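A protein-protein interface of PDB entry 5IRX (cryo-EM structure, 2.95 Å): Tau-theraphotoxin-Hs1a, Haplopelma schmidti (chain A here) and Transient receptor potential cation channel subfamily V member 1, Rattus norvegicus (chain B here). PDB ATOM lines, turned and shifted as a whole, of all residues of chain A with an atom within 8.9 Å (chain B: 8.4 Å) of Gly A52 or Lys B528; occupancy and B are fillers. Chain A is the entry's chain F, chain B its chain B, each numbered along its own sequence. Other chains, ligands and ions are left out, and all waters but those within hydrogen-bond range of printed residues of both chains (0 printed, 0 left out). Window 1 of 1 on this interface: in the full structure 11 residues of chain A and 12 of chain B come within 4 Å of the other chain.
The backbone NH (N) of Phe B527 lies close to the backbone carbonyl oxygen (O) of Trp A53, at 3.4 Å.
The backbone NH (N) of Ala B529 lies within hydrogen-bond range of the backbone carbonyl oxygen (O) of Gly A52, at 2.7 Å.
The backbone NH (N) of Lys B528 sits at hydrogen-bond distance from the backbone carbonyl oxygen (O) of Gly A52.
O of Glu B523 is in hydrogen-bond range of NZ of Lys B528, 3.3 Å away.
N of Gly A52 lies within hydrogen-bond range of SG of Cys A63.
The backbone NH of Ala A45 sits at hydrogen-bond distance from the backbone carbonyl oxygen of Lys A56 (2.9 Å).
O of Phe A67 lies within hydrogen-bond range of NE1 of Trp A53 (2.9 Å).
The side-chain sulfur (SG) of Cys A57 is disulfide-bonded to the side-chain sulfur (SG) of Cys A71 (2.0 Å).
The side-chain sulfur (SG) of Cys A51 is disulfide-bonded to the side-chain sulfur (SG) of Cys A63 (2.0 Å).
Among the printed residues, merely in contact across the chains: Gly A52 with Tyr B525, Gly A52 with Phe B527, Gly A52 with Val B530, Trp A53 with Ala B529, Trp A53 with Val B530, Gly A54 with Asp B526, Gly A54 with Phe B527, Lys A56 with Tyr B525, Lys A56 with Asp B526, Pro A64 with Lys B528, Leu A65 with Ile B532, Phe A67 with Ala B529 and Phe A67 with Ile B533.
Printed residues of chain B within 4 Å of Gly A52: Tyr B525 (3.97 Å), Phe B527 (3.3 Å), Lys B528 (2.7 Å), Ala B529 (2.7 Å) and Val B530 (3.996 Å).
Lys B528 touches just these residues of chain A: Gly A52 and Pro A64.
No residue of chain B comes within 4 Å of Cys A51.
Ala B529 touches just these residues of chain A: Gly A52, Trp A53 and Phe A67.
Of the printed residues of chain A, Ile B532 touches Leu A65 (3.7 Å).
Printed residues of chain B within 4 Å of Lys A56: Tyr B525 and Asp B526.
Of the printed residues of chain A, Tyr B525 touches Gly A52 and Lys A56.
Printed residues of chain B within 4 Å of Trp A53: Phe B527, Ala B529 and Val B530.
The nearest printed residue of chain B that does not touch Gly A52 is Asp B526 (4.7 Å).
The nearest residue of chain A that does not touch Lys B528 is Trp A53 (4.6 Å).
The nearest printed residue of chain A that does not touch Asp B526 is Ser A55 (4.1 Å).
Of the 18 printed residues of chain B, 8 touch a printed residue of chain A.
Hydrophobic or aromatic side chains of chain A that line the printed part of chain B: Trp A53, Leu A65 and Phe A67.
Among the printed residues, no Asp or Glu carboxylate lies within 4 Å of a Lys or Arg side-chain nitrogen of the other chain.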
ATOM      1  N   ALA A  45     -30.585 -33.595  -7.345  1.00  0.00           N
ATOM      2  CA  ALA A  45     -29.418 -34.253  -6.784  1.00  0.00           C
ATOM      3  C   ALA A  45     -29.874 -35.527  -6.093  1.00  0.00           C
ATOM      4  O   ALA A  45     -30.711 -35.481  -5.189  1.00  0.00           O
ATOM      5  CB  ALA A  45     -28.685 -33.336  -5.808  1.00  0.00           C
ATOM      6  N   GLU A  49     -25.487 -37.534  -3.125  1.00  0.00           N
ATOM      7  CA  GLU A  49     -24.922 -36.430  -3.877  1.00  0.00           C
ATOM      8  C   GLU A  49     -25.061 -35.154  -3.065  1.00  0.00           C
ATOM      9  O   GLU A  49     -25.816 -35.099  -2.091  1.00  0.00           O
ATOM     10  CB  GLU A  49     -25.614 -36.264  -5.225  1.00  0.00           C
ATOM     11  CG  GLU A  49     -25.338 -37.381  -6.201  1.00  0.00           C
ATOM     12  CD  GLU A  49     -26.078 -37.192  -7.505  1.00  0.00           C
ATOM     13  OE1 GLU A  49     -26.933 -36.287  -7.575  1.00  0.00           O
ATOM     14  OE2 GLU A  49     -25.795 -37.935  -8.465  1.00  0.00           O
ATOM     15  N   VAL A  50     -24.324 -34.124  -3.476  1.00  0.00           N
ATOM     16  CA  VAL A  50     -24.332 -32.879  -2.729  1.00  0.00           C
ATOM     17  C   VAL A  50     -25.602 -32.111  -3.033  1.00  0.00           C
ATOM     18  O   VAL A  50     -25.873 -31.753  -4.183  1.00  0.00           O
ATOM     19  CB  VAL A  50     -23.091 -32.048  -3.064  1.00  0.00           C
ATOM     20  CG1 VAL A  50     -23.164 -30.724  -2.364  1.00  0.00           C
ATOM     21  CG2 VAL A  50     -21.853 -32.781  -2.648  1.00  0.00           C
ATOM     22  N   CYS A  51     -26.391 -31.861  -2.000  1.00  0.00           N
ATOM     23  CA  CYS A  51     -27.549 -30.992  -2.077  1.00  0.00           C
ATOM     24  C   CYS A  51     -27.210 -29.674  -1.410  1.00  0.00           C
ATOM     25  O   CYS A  51     -26.225 -29.555  -0.682  1.00  0.00           O
ATOM     26  CB  CYS A  51     -28.764 -31.628  -1.403  1.00  0.00           C
ATOM     27  SG  CYS A  51     -28.496 -31.972   0.339  1.00  0.00           S
ATOM     28  N   GLY A  52     -28.037 -28.671  -1.667  1.00  0.00           N
ATOM     29  CA  GLY A  52     -27.883 -27.400  -1.009  1.00  0.00           C
ATOM     30  C   GLY A  52     -26.841 -26.483  -1.595  1.00  0.00           C
ATOM     31  O   GLY A  52     -26.759 -25.328  -1.174  1.00  0.00           O
ATOM     32  N   TRP A  53     -26.015 -26.956  -2.524  1.00  0.00           N
ATOM     33  CA  TRP A  53     -25.133 -26.079  -3.277  1.00  0.00           C
ATOM     34  C   TRP A  53     -25.547 -26.010  -4.737  1.00  0.00           C
ATOM     35  O   TRP A  53     -26.038 -24.986  -5.190  1.00  0.00           O
ATOM     36  CB  TRP A  53     -23.688 -26.564  -3.165  1.00  0.00           C
ATOM     37  CG  TRP A  53     -23.130 -26.404  -1.817  1.00  0.00           C
ATOM     38  CD1 TRP A  53     -23.237 -27.274  -0.791  1.00  0.00           C
ATOM     39  CD2 TRP A  53     -22.316 -25.334  -1.354  1.00  0.00           C
ATOM     40  NE1 TRP A  53     -22.571 -26.800   0.304  1.00  0.00           N
ATOM     41  CE2 TRP A  53     -21.992 -25.607  -0.021  1.00  0.00           C
ATOM     42  CE3 TRP A  53     -21.835 -24.164  -1.935  1.00  0.00           C
ATOM     43  CZ2 TRP A  53     -21.219 -24.757   0.741  1.00  0.00           C
ATOM     44  CZ3 TRP A  53     -21.068 -23.320  -1.176  1.00  0.00           C
ATOM     45  CH2 TRP A  53     -20.768 -23.617   0.146  1.00  0.00           C
ATOM     46  N   GLY A  54     -25.462 -27.103  -5.464  1.00  0.00           N
ATOM     47  CA  GLY A  54     -25.830 -27.021  -6.856  1.00  0.00           C
ATOM     48  C   GLY A  54     -27.312 -27.211  -7.061  1.00  0.00           C
ATOM     49  O   GLY A  54     -27.994 -26.337  -7.601  1.00  0.00           O
ATOM     50  N   SER A  55     -27.826 -28.343  -6.603  1.00  0.00           N
ATOM     51  CA  SER A  55     -29.170 -28.762  -6.937  1.00  0.00           C
ATOM     52  C   SER A  55     -29.948 -29.065  -5.671  1.00  0.00           C
ATOM     53  O   SER A  55     -29.373 -29.315  -4.612  1.00  0.00           O
ATOM     54  CB  SER A  55     -29.145 -29.995  -7.840  1.00  0.00           C
ATOM     55  N   LYS A  56     -31.270 -29.028  -5.801  1.00  0.00           N
ATOM     56  CA  LYS A  56     -32.144 -29.485  -4.738  1.00  0.00           C
ATOM     57  C   LYS A  56     -31.956 -30.970  -4.509  1.00  0.00           C
ATOM     58  O   LYS A  56     -31.539 -31.717  -5.394  1.00  0.00           O
ATOM     59  CB  LYS A  56     -33.607 -29.258  -5.092  1.00  0.00           C
ATOM     60  CG  LYS A  56     -34.038 -27.838  -5.200  1.00  0.00           C
ATOM     61  CD  LYS A  56     -35.505 -27.785  -5.542  1.00  0.00           C
ATOM     62  CE  LYS A  56     -35.971 -26.362  -5.723  1.00  0.00           C
ATOM     63  NZ  LYS A  56     -37.408 -26.313  -6.092  1.00  0.00           N
ATOM     64  N   CYS A  57     -32.292 -31.409  -3.310  1.00  0.00           N
ATOM     65  CA  CYS A  57     -32.411 -32.834  -3.103  1.00  0.00           C
ATOM     66  C   CYS A  57     -33.782 -33.261  -3.604  1.00  0.00           C
ATOM     67  O   CYS A  57     -34.709 -32.452  -3.680  1.00  0.00           O
ATOM     68  CB  CYS A  57     -32.218 -33.187  -1.634  1.00  0.00           C
ATOM     69  SG  CYS A  57     -31.939 -34.920  -1.437  1.00  0.00           S
ATOM     70  N   CYS A  58     -33.907 -34.534  -3.976  1.00  0.00           N
ATOM     71  CA  CYS A  58     -35.101 -34.992  -4.678  1.00  0.00           C
ATOM     72  C   CYS A  58     -36.274 -35.152  -3.709  1.00  0.00           C
ATOM     73  O   CYS A  58     -36.229 -34.738  -2.547  1.00  0.00           O
ATOM     74  CB  CYS A  58     -34.826 -36.302  -5.407  1.00  0.00           C
ATOM     75  SG  CYS A  58     -33.515 -36.195  -6.635  1.00  0.00           S
ATOM     76  N   ASP A  62     -34.120 -36.059   2.278  1.00  0.00           N
ATOM     77  CA  ASP A  62     -33.826 -34.756   2.843  1.00  0.00           C
ATOM     78  C   ASP A  62     -32.400 -34.340   2.496  1.00  0.00           C
ATOM     79  O   ASP A  62     -31.583 -35.143   2.040  1.00  0.00           O
ATOM     80  CB  ASP A  62     -34.054 -34.753   4.356  1.00  0.00           C
ATOM     81  CG  ASP A  62     -33.225 -35.797   5.098  1.00  0.00           C
ATOM     82  OD1 ASP A  62     -32.554 -36.628   4.462  1.00  0.00           O
ATOM     83  OD2 ASP A  62     -33.249 -35.788   6.345  1.00  0.00           O
ATOM     84  N   CYS A  63     -32.107 -33.065   2.703  1.00  0.00           N
ATOM     85  CA  CYS A  63     -30.769 -32.571   2.408  1.00  0.00           C
ATOM     86  C   CYS A  63     -29.802 -32.880   3.561  1.00  0.00           C
ATOM     87  O   CYS A  63     -28.675 -33.302   3.293  1.00  0.00           O
ATOM     88  CB  CYS A  63     -30.833 -31.082   2.047  1.00  0.00           C
ATOM     89  SG  CYS A  63     -29.327 -30.411   1.338  1.00  0.00           S
ATOM     90  N   PRO A  64     -30.155 -32.673   4.845  1.00  0.00           N
ATOM     91  CA  PRO A  64     -31.094 -31.807   5.556  1.00  0.00           C
ATOM     92  C   PRO A  64     -30.442 -30.540   6.066  1.00  0.00           C
ATOM     93  O   PRO A  64     -30.971 -29.469   5.779  1.00  0.00           O
ATOM     94  CB  PRO A  64     -31.557 -32.682   6.719  1.00  0.00           C
ATOM     95  N   LEU A  65     -29.283 -30.646   6.720  1.00  0.00           N
ATOM     96  CA  LEU A  65     -28.599 -29.474   7.261  1.00  0.00           C
ATOM     97  C   LEU A  65     -27.176 -29.853   7.625  1.00  0.00           C
ATOM     98  O   LEU A  65     -26.951 -30.538   8.625  1.00  0.00           O
ATOM     99  CB  LEU A  65     -29.338 -28.915   8.474  1.00  0.00           C
ATOM    100  CG  LEU A  65     -28.855 -27.582   9.014  1.00  0.00           C
ATOM    101  CD1 LEU A  65     -28.881 -26.577   7.912  1.00  0.00           C
ATOM    102  CD2 LEU A  65     -29.807 -27.150  10.089  1.00  0.00           C
ATOM    103  N   ALA A  66     -26.226 -29.366   6.843  1.00  0.00           N
ATOM    104  CA  ALA A  66     -24.804 -29.536   7.087  1.00  0.00           C
ATOM    105  C   ALA A  66     -24.108 -28.476   6.259  1.00  0.00           C
ATOM    106  O   ALA A  66     -24.754 -27.699   5.557  1.00  0.00           O
ATOM    107  CB  ALA A  66     -24.317 -30.939   6.724  1.00  0.00           C
ATOM    108  N   PHE A  67     -22.783 -28.432   6.350  1.00  0.00           N
ATOM    109  CA  PHE A  67     -22.065 -27.464   5.536  1.00  0.00           C
ATOM    110  C   PHE A  67     -22.009 -27.926   4.091  1.00  0.00           C
ATOM    111  O   PHE A  67     -22.460 -27.223   3.184  1.00  0.00           O
ATOM    112  CB  PHE A  67     -20.668 -27.219   6.085  1.00  0.00           C
ATOM    113  CG  PHE A  67     -19.914 -26.189   5.322  1.00  0.00           C
ATOM    114  CD1 PHE A  67     -20.268 -24.863   5.409  1.00  0.00           C
ATOM    115  CD2 PHE A  67     -18.855 -26.541   4.516  1.00  0.00           C
ATOM    116  CE1 PHE A  67     -19.585 -23.908   4.702  1.00  0.00           C
ATOM    117  CE2 PHE A  67     -18.166 -25.587   3.812  1.00  0.00           C
ATOM    118  CZ  PHE A  67     -18.534 -24.270   3.905  1.00  0.00           C
ATOM    119  N   ILE A  68     -21.473 -29.113   3.859  1.00  0.00           N
ATOM    120  CA  ILE A  68     -21.605 -29.742   2.554  1.00  0.00           C
ATOM    121  C   ILE A  68     -22.614 -30.865   2.738  1.00  0.00           C
ATOM    122  O   ILE A  68     -22.254 -31.965   3.174  1.00  0.00           O
ATOM    123  CB  ILE A  68     -20.255 -30.236   2.028  1.00  0.00           C
ATOM    124  CG1 ILE A  68     -19.309 -29.054   1.882  1.00  0.00           C
ATOM    125  CG2 ILE A  68     -20.419 -30.887   0.681  1.00  0.00           C
ATOM    126  CD1 ILE A  68     -17.906 -29.448   1.544  1.00  0.00           C
ATOM    127  N   PRO A  69     -23.874 -30.625   2.455  1.00  0.00           N
ATOM    128  CA  PRO A  69     -24.891 -31.615   2.811  1.00  0.00           C
ATOM    129  C   PRO A  69     -25.091 -32.668   1.737  1.00  0.00           C
ATOM    130  O   PRO A  69     -25.234 -32.346   0.556  1.00  0.00           O
ATOM    131  CB  PRO A  69     -26.143 -30.759   3.005  1.00  0.00           C
ATOM    132  N   TYR A  70     -25.098 -33.931   2.139  1.00  0.00           N
ATOM    133  CA  TYR A  70     -25.387 -35.044   1.249  1.00  0.00           C
ATOM    134  C   TYR A  70     -26.800 -35.531   1.505  1.00  0.00           C
ATOM    135  O   TYR A  70     -27.217 -35.622   2.662  1.00  0.00           O
ATOM    136  CB  TYR A  70     -24.410 -36.188   1.477  1.00  0.00           C
ATOM    137  CG  TYR A  70     -23.006 -35.877   1.078  1.00  0.00           C
ATOM    138  CD1 TYR A  70     -22.610 -35.979  -0.240  1.00  0.00           C
ATOM    139  CD2 TYR A  70     -22.072 -35.486   2.018  1.00  0.00           C
ATOM    140  CE1 TYR A  70     -21.325 -35.705  -0.615  1.00  0.00           C
ATOM    141  CE2 TYR A  70     -20.782 -35.206   1.654  1.00  0.00           C
ATOM    142  CZ  TYR A  70     -20.414 -35.314   0.333  1.00  0.00           C
ATOM    143  OH  TYR A  70     -19.125 -35.035  -0.048  1.00  0.00           O
ATOM    144  N   CYS A  71     -27.522 -35.863   0.435  1.00  0.00           N
ATOM    145  CA  CYS A  71     -28.879 -36.375   0.566  1.00  0.00           C
ATOM    146  C   CYS A  71     -28.889 -37.711   1.296  1.00  0.00           C
ATOM    147  O   CYS A  71     -27.910 -38.461   1.300  1.00  0.00           O
ATOM    148  CB  CYS A  71     -29.536 -36.564  -0.795  1.00  0.00           C
ATOM    149  SG  CYS A  71     -29.941 -35.099  -1.724  1.00  0.00           S
ATOM    150  N   LEU B 493     -30.286 -15.603  -5.951  1.00  0.00           N
ATOM    151  CA  LEU B 493     -29.741 -16.855  -5.456  1.00  0.00           C
ATOM    152  C   LEU B 493     -30.789 -17.946  -5.502  1.00  0.00           C
ATOM    153  O   LEU B 493     -30.584 -18.997  -6.113  1.00  0.00           O
ATOM    154  CB  LEU B 493     -29.227 -16.686  -4.034  1.00  0.00           C
ATOM    155  CG  LEU B 493     -28.539 -17.916  -3.472  1.00  0.00           C
ATOM    156  CD1 LEU B 493     -27.285 -18.165  -4.236  1.00  0.00           C
ATOM    157  CD2 LEU B 493     -28.234 -17.713  -2.026  1.00  0.00           C
ATOM    158  N   ILE B 494     -31.919 -17.724  -4.853  1.00  0.00           N
ATOM    159  CA  ILE B 494     -32.967 -18.724  -4.787  1.00  0.00           C
ATOM    160  C   ILE B 494     -34.243 -18.141  -5.368  1.00  0.00           C
ATOM    161  O   ILE B 494     -34.604 -16.994  -5.089  1.00  0.00           O
ATOM    162  CB  ILE B 494     -33.144 -19.249  -3.345  1.00  0.00           C
ATOM    163  CG1 ILE B 494     -33.430 -18.155  -2.336  1.00  0.00           C
ATOM    164  CG2 ILE B 494     -31.907 -19.949  -2.880  1.00  0.00           C
ATOM    165  CD1 ILE B 494     -34.841 -18.085  -1.992  1.00  0.00           C
ATOM    166  N   GLU B 520     -35.515 -20.031  10.247  1.00  0.00           N
ATOM    167  CA  GLU B 520     -35.849 -21.439  10.115  1.00  0.00           C
ATOM    168  C   GLU B 520     -35.411 -21.847   8.720  1.00  0.00           C
ATOM    169  O   GLU B 520     -35.991 -21.412   7.724  1.00  0.00           O
ATOM    170  CB  GLU B 520     -37.336 -21.680  10.341  1.00  0.00           C
ATOM    171  N   PHE B 521     -34.389 -22.687   8.652  1.00  0.00           N
ATOM    172  CA  PHE B 521     -33.826 -23.119   7.379  1.00  0.00           C
ATOM    173  C   PHE B 521     -34.393 -24.453   6.960  1.00  0.00           C
ATOM    174  O   PHE B 521     -33.666 -25.342   6.521  1.00  0.00           O
ATOM    175  CB  PHE B 521     -32.311 -23.179   7.469  1.00  0.00           C
ATOM    176  CG  PHE B 521     -31.687 -21.884   7.858  1.00  0.00           C
ATOM    177  CD1 PHE B 521     -31.685 -20.815   6.984  1.00  0.00           C
ATOM    178  CD2 PHE B 521     -31.070 -21.743   9.087  1.00  0.00           C
ATOM    179  CE1 PHE B 521     -31.106 -19.618   7.340  1.00  0.00           C
ATOM    180  CE2 PHE B 521     -30.481 -20.552   9.445  1.00  0.00           C
ATOM    181  CZ  PHE B 521     -30.502 -19.487   8.571  1.00  0.00           C
ATOM    182  N   THR B 522     -35.697 -24.621   7.161  1.00  0.00           N
ATOM    183  CA  THR B 522     -36.352 -25.897   6.918  1.00  0.00           C
ATOM    184  C   THR B 522     -36.365 -26.250   5.439  1.00  0.00           C
ATOM    185  O   THR B 522     -35.840 -27.293   5.035  1.00  0.00           O
ATOM    186  CB  THR B 522     -37.779 -25.852   7.453  1.00  0.00           C
ATOM    187  OG1 THR B 522     -38.510 -24.839   6.755  1.00  0.00           O
ATOM    188  CG2 THR B 522     -37.775 -25.530   8.931  1.00  0.00           C
ATOM    189  N   GLU B 523     -36.956 -25.390   4.614  1.00  0.00           N
ATOM    190  CA  GLU B 523     -37.347 -25.804   3.277  1.00  0.00           C
ATOM    191  C   GLU B 523     -36.155 -25.888   2.339  1.00  0.00           C
ATOM    192  O   GLU B 523     -35.162 -25.174   2.487  1.00  0.00           O
ATOM    193  CB  GLU B 523     -38.404 -24.866   2.709  1.00  0.00           C
ATOM    194  CG  GLU B 523     -37.981 -23.445   2.543  1.00  0.00           C
ATOM    195  CD  GLU B 523     -39.113 -22.602   2.006  1.00  0.00           C
ATOM    196  OE1 GLU B 523     -40.204 -23.162   1.776  1.00  0.00           O
ATOM    197  OE2 GLU B 523     -38.925 -21.386   1.813  1.00  0.00           O
ATOM    198  N   ASN B 524     -36.260 -26.800   1.381  1.00  0.00           N
ATOM    199  CA  ASN B 524     -35.137 -27.167   0.535  1.00  0.00           C
ATOM    200  C   ASN B 524     -35.024 -26.188  -0.619  1.00  0.00           C
ATOM    201  O   ASN B 524     -35.996 -25.956  -1.342  1.00  0.00           O
ATOM    202  CB  ASN B 524     -35.313 -28.588   0.013  1.00  0.00           C
ATOM    203  N   TYR B 525     -33.845 -25.612  -0.786  1.00  0.00           N
ATOM    204  CA  TYR B 525     -33.533 -24.810  -1.951  1.00  0.00           C
ATOM    205  C   TYR B 525     -32.322 -25.404  -2.644  1.00  0.00           C
ATOM    206  O   TYR B 525     -31.462 -26.014  -2.007  1.00  0.00           O
ATOM    207  CB  TYR B 525     -33.191 -23.374  -1.593  1.00  0.00           C
ATOM    208  CG  TYR B 525     -34.227 -22.600  -0.839  1.00  0.00           C
ATOM    209  CD1 TYR B 525     -35.353 -22.116  -1.466  1.00  0.00           C
ATOM    210  CD2 TYR B 525     -34.032 -22.285   0.489  1.00  0.00           C
ATOM    211  CE1 TYR B 525     -36.281 -21.390  -0.775  1.00  0.00           C
ATOM    212  CE2 TYR B 525     -34.944 -21.561   1.182  1.00  0.00           C
ATOM    213  CZ  TYR B 525     -36.065 -21.114   0.548  1.00  0.00           C
ATOM    214  OH  TYR B 525     -36.981 -20.382   1.252  1.00  0.00           O
ATOM    215  N   ASP B 526     -32.245 -25.215  -3.949  1.00  0.00           N
ATOM    216  CA  ASP B 526     -30.935 -25.195  -4.561  1.00  0.00           C
ATOM    217  C   ASP B 526     -30.242 -23.957  -4.038  1.00  0.00           C
ATOM    218  O   ASP B 526     -30.884 -22.917  -3.875  1.00  0.00           O
ATOM    219  CB  ASP B 526     -31.039 -25.160  -6.080  1.00  0.00           C
ATOM    220  N   PHE B 527     -28.948 -24.086  -3.741  1.00  0.00           N
ATOM    221  CA  PHE B 527     -28.147 -23.061  -3.062  1.00  0.00           C
ATOM    222  C   PHE B 527     -28.715 -22.751  -1.685  1.00  0.00           C
ATOM    223  O   PHE B 527     -28.879 -21.600  -1.300  1.00  0.00           O
ATOM    224  CB  PHE B 527     -27.995 -21.791  -3.903  1.00  0.00           C
ATOM    225  CG  PHE B 527     -27.270 -22.021  -5.160  1.00  0.00           C
ATOM    226  CD1 PHE B 527     -25.896 -21.984  -5.187  1.00  0.00           C
ATOM    227  CD2 PHE B 527     -27.956 -22.339  -6.308  1.00  0.00           C
ATOM    228  CE1 PHE B 527     -25.225 -22.238  -6.345  1.00  0.00           C
ATOM    229  CE2 PHE B 527     -27.291 -22.591  -7.459  1.00  0.00           C
ATOM    230  CZ  PHE B 527     -25.923 -22.562  -7.474  1.00  0.00           C
ATOM    231  N   LYS B 528     -29.013 -23.807  -0.938  1.00  0.00           N
ATOM    232  CA  LYS B 528     -29.446 -23.657   0.441  1.00  0.00           C
ATOM    233  C   LYS B 528     -28.275 -23.378   1.363  1.00  0.00           C
ATOM    234  O   LYS B 528     -28.383 -22.552   2.270  1.00  0.00           O
ATOM    235  CB  LYS B 528     -30.168 -24.917   0.892  1.00  0.00           C
ATOM    236  CG  LYS B 528     -30.598 -24.927   2.322  1.00  0.00           C
ATOM    237  CD  LYS B 528     -31.268 -26.230   2.646  1.00  0.00           C
ATOM    238  CE  LYS B 528     -31.573 -26.311   4.108  1.00  0.00           C
ATOM    239  NZ  LYS B 528     -32.551 -25.259   4.436  1.00  0.00           N
ATOM    240  N   ALA B 529     -27.154 -24.057   1.149  1.00  0.00           N
ATOM    241  CA  ALA B 529     -26.005 -23.858   2.019  1.00  0.00           C
ATOM    242  C   ALA B 529     -25.350 -22.513   1.784  1.00  0.00           C
ATOM    243  O   ALA B 529     -24.755 -21.951   2.705  1.00  0.00           O
ATOM    244  CB  ALA B 529     -24.994 -24.973   1.817  1.00  0.00           C
ATOM    245  N   VAL B 530     -25.440 -21.983   0.569  1.00  0.00           N
ATOM    246  CA  VAL B 530     -24.966 -20.628   0.333  1.00  0.00           C
ATOM    247  C   VAL B 530     -25.900 -19.642   0.989  1.00  0.00           C
ATOM    248  O   VAL B 530     -25.463 -18.636   1.552  1.00  0.00           O
ATOM    249  CB  VAL B 530     -24.858 -20.367  -1.172  1.00  0.00           C
ATOM    250  CG1 VAL B 530     -24.298 -19.006  -1.438  1.00  0.00           C
ATOM    251  CG2 VAL B 530     -24.013 -21.402  -1.795  1.00  0.00           C
ATOM    252  N   PHE B 531     -27.195 -19.934   0.955  1.00  0.00           N
ATOM    253  CA  PHE B 531     -28.205 -19.058   1.519  1.00  0.00           C
ATOM    254  C   PHE B 531     -28.063 -18.902   3.020  1.00  0.00           C
ATOM    255  O   PHE B 531     -28.342 -17.832   3.553  1.00  0.00           O
ATOM    256  CB  PHE B 531     -29.575 -19.604   1.170  1.00  0.00           C
ATOM    257  CG  PHE B 531     -30.690 -18.856   1.772  1.00  0.00           C
ATOM    258  CD1 PHE B 531     -31.006 -17.599   1.328  1.00  0.00           C
ATOM    259  CD2 PHE B 531     -31.452 -19.428   2.757  1.00  0.00           C
ATOM    260  CE1 PHE B 531     -32.042 -16.917   1.878  1.00  0.00           C
ATOM    261  CE2 PHE B 531     -32.489 -18.752   3.306  1.00  0.00           C
ATOM    262  CZ  PHE B 531     -32.787 -17.495   2.864  1.00  0.00           C
ATOM    263  N   ILE B 532     -27.615 -19.945   3.712  1.00  0.00           N
ATOM    264  CA  ILE B 532     -27.370 -19.835   5.141  1.00  0.00           C
ATOM    265  C   ILE B 532     -26.148 -18.971   5.409  1.00  0.00           C
ATOM    266  O   ILE B 532     -26.112 -18.226   6.392  1.00  0.00           O
ATOM    267  CB  ILE B 532     -27.246 -21.246   5.733  1.00  0.00           C
ATOM    268  CG1 ILE B 532     -28.574 -21.958   5.585  1.00  0.00           C
ATOM    269  CG2 ILE B 532     -26.865 -21.230   7.182  1.00  0.00           C
ATOM    270  CD1 ILE B 532     -28.530 -23.387   5.976  1.00  0.00           C
ATOM    271  N   ILE B 533     -25.156 -19.007   4.524  1.00  0.00           N
ATOM    272  CA  ILE B 533     -23.950 -18.222   4.745  1.00  0.00           C
ATOM    273  C   ILE B 533     -24.225 -16.744   4.536  1.00  0.00           C
ATOM    274  O   ILE B 533     -23.732 -15.909   5.294  1.00  0.00           O
ATOM    275  CB  ILE B 533     -22.811 -18.732   3.850  1.00  0.00           C
ATOM    276  CG1 ILE B 533     -22.474 -20.162   4.221  1.00  0.00           C
ATOM    277  CG2 ILE B 533     -21.563 -17.922   4.032  1.00  0.00           C
ATOM    278  CD1 ILE B 533     -21.503 -20.796   3.280  1.00  0.00           C
ATOM    279  N   LEU B 534     -25.039 -16.393   3.538  1.00  0.00           N
ATOM    280  CA  LEU B 534     -25.424 -14.995   3.363  1.00  0.00           C
ATOM    281  C   LEU B 534     -26.278 -14.509   4.509  1.00  0.00           C
ATOM    282  O   LEU B 534     -26.050 -13.427   5.054  1.00  0.00           O
ATOM    283  CB  LEU B 534     -26.215 -14.786   2.085  1.00  0.00           C
ATOM    284  CG  LEU B 534     -25.659 -14.799   0.694  1.00  0.00           C
ATOM    285  CD1 LEU B 534     -26.849 -14.602  -0.170  1.00  0.00           C
ATOM    286  CD2 LEU B 534     -24.717 -13.657   0.538  1.00  0.00           C
ATOM    287  N   LEU B 535     -27.287 -15.286   4.866  1.00  0.00           N
ATOM    288  CA  LEU B 535     -28.278 -14.806   5.806  1.00  0.00           C
ATOM    289  C   LEU B 535     -27.715 -14.747   7.211  1.00  0.00           C
ATOM    290  O   LEU B 535     -28.185 -13.958   8.029  1.00  0.00           O
ATOM    291  CB  LEU B 535     -29.492 -15.708   5.739  1.00  0.00           C
ATOM    292  CG  LEU B 535     -30.747 -15.175   6.375  1.00  0.00           C
ATOM    293  CD1 LEU B 535     -31.121 -13.951   5.607  1.00  0.00           C
ATOM    294  CD2 LEU B 535     -31.799 -16.217   6.260  1.00  0.00           C
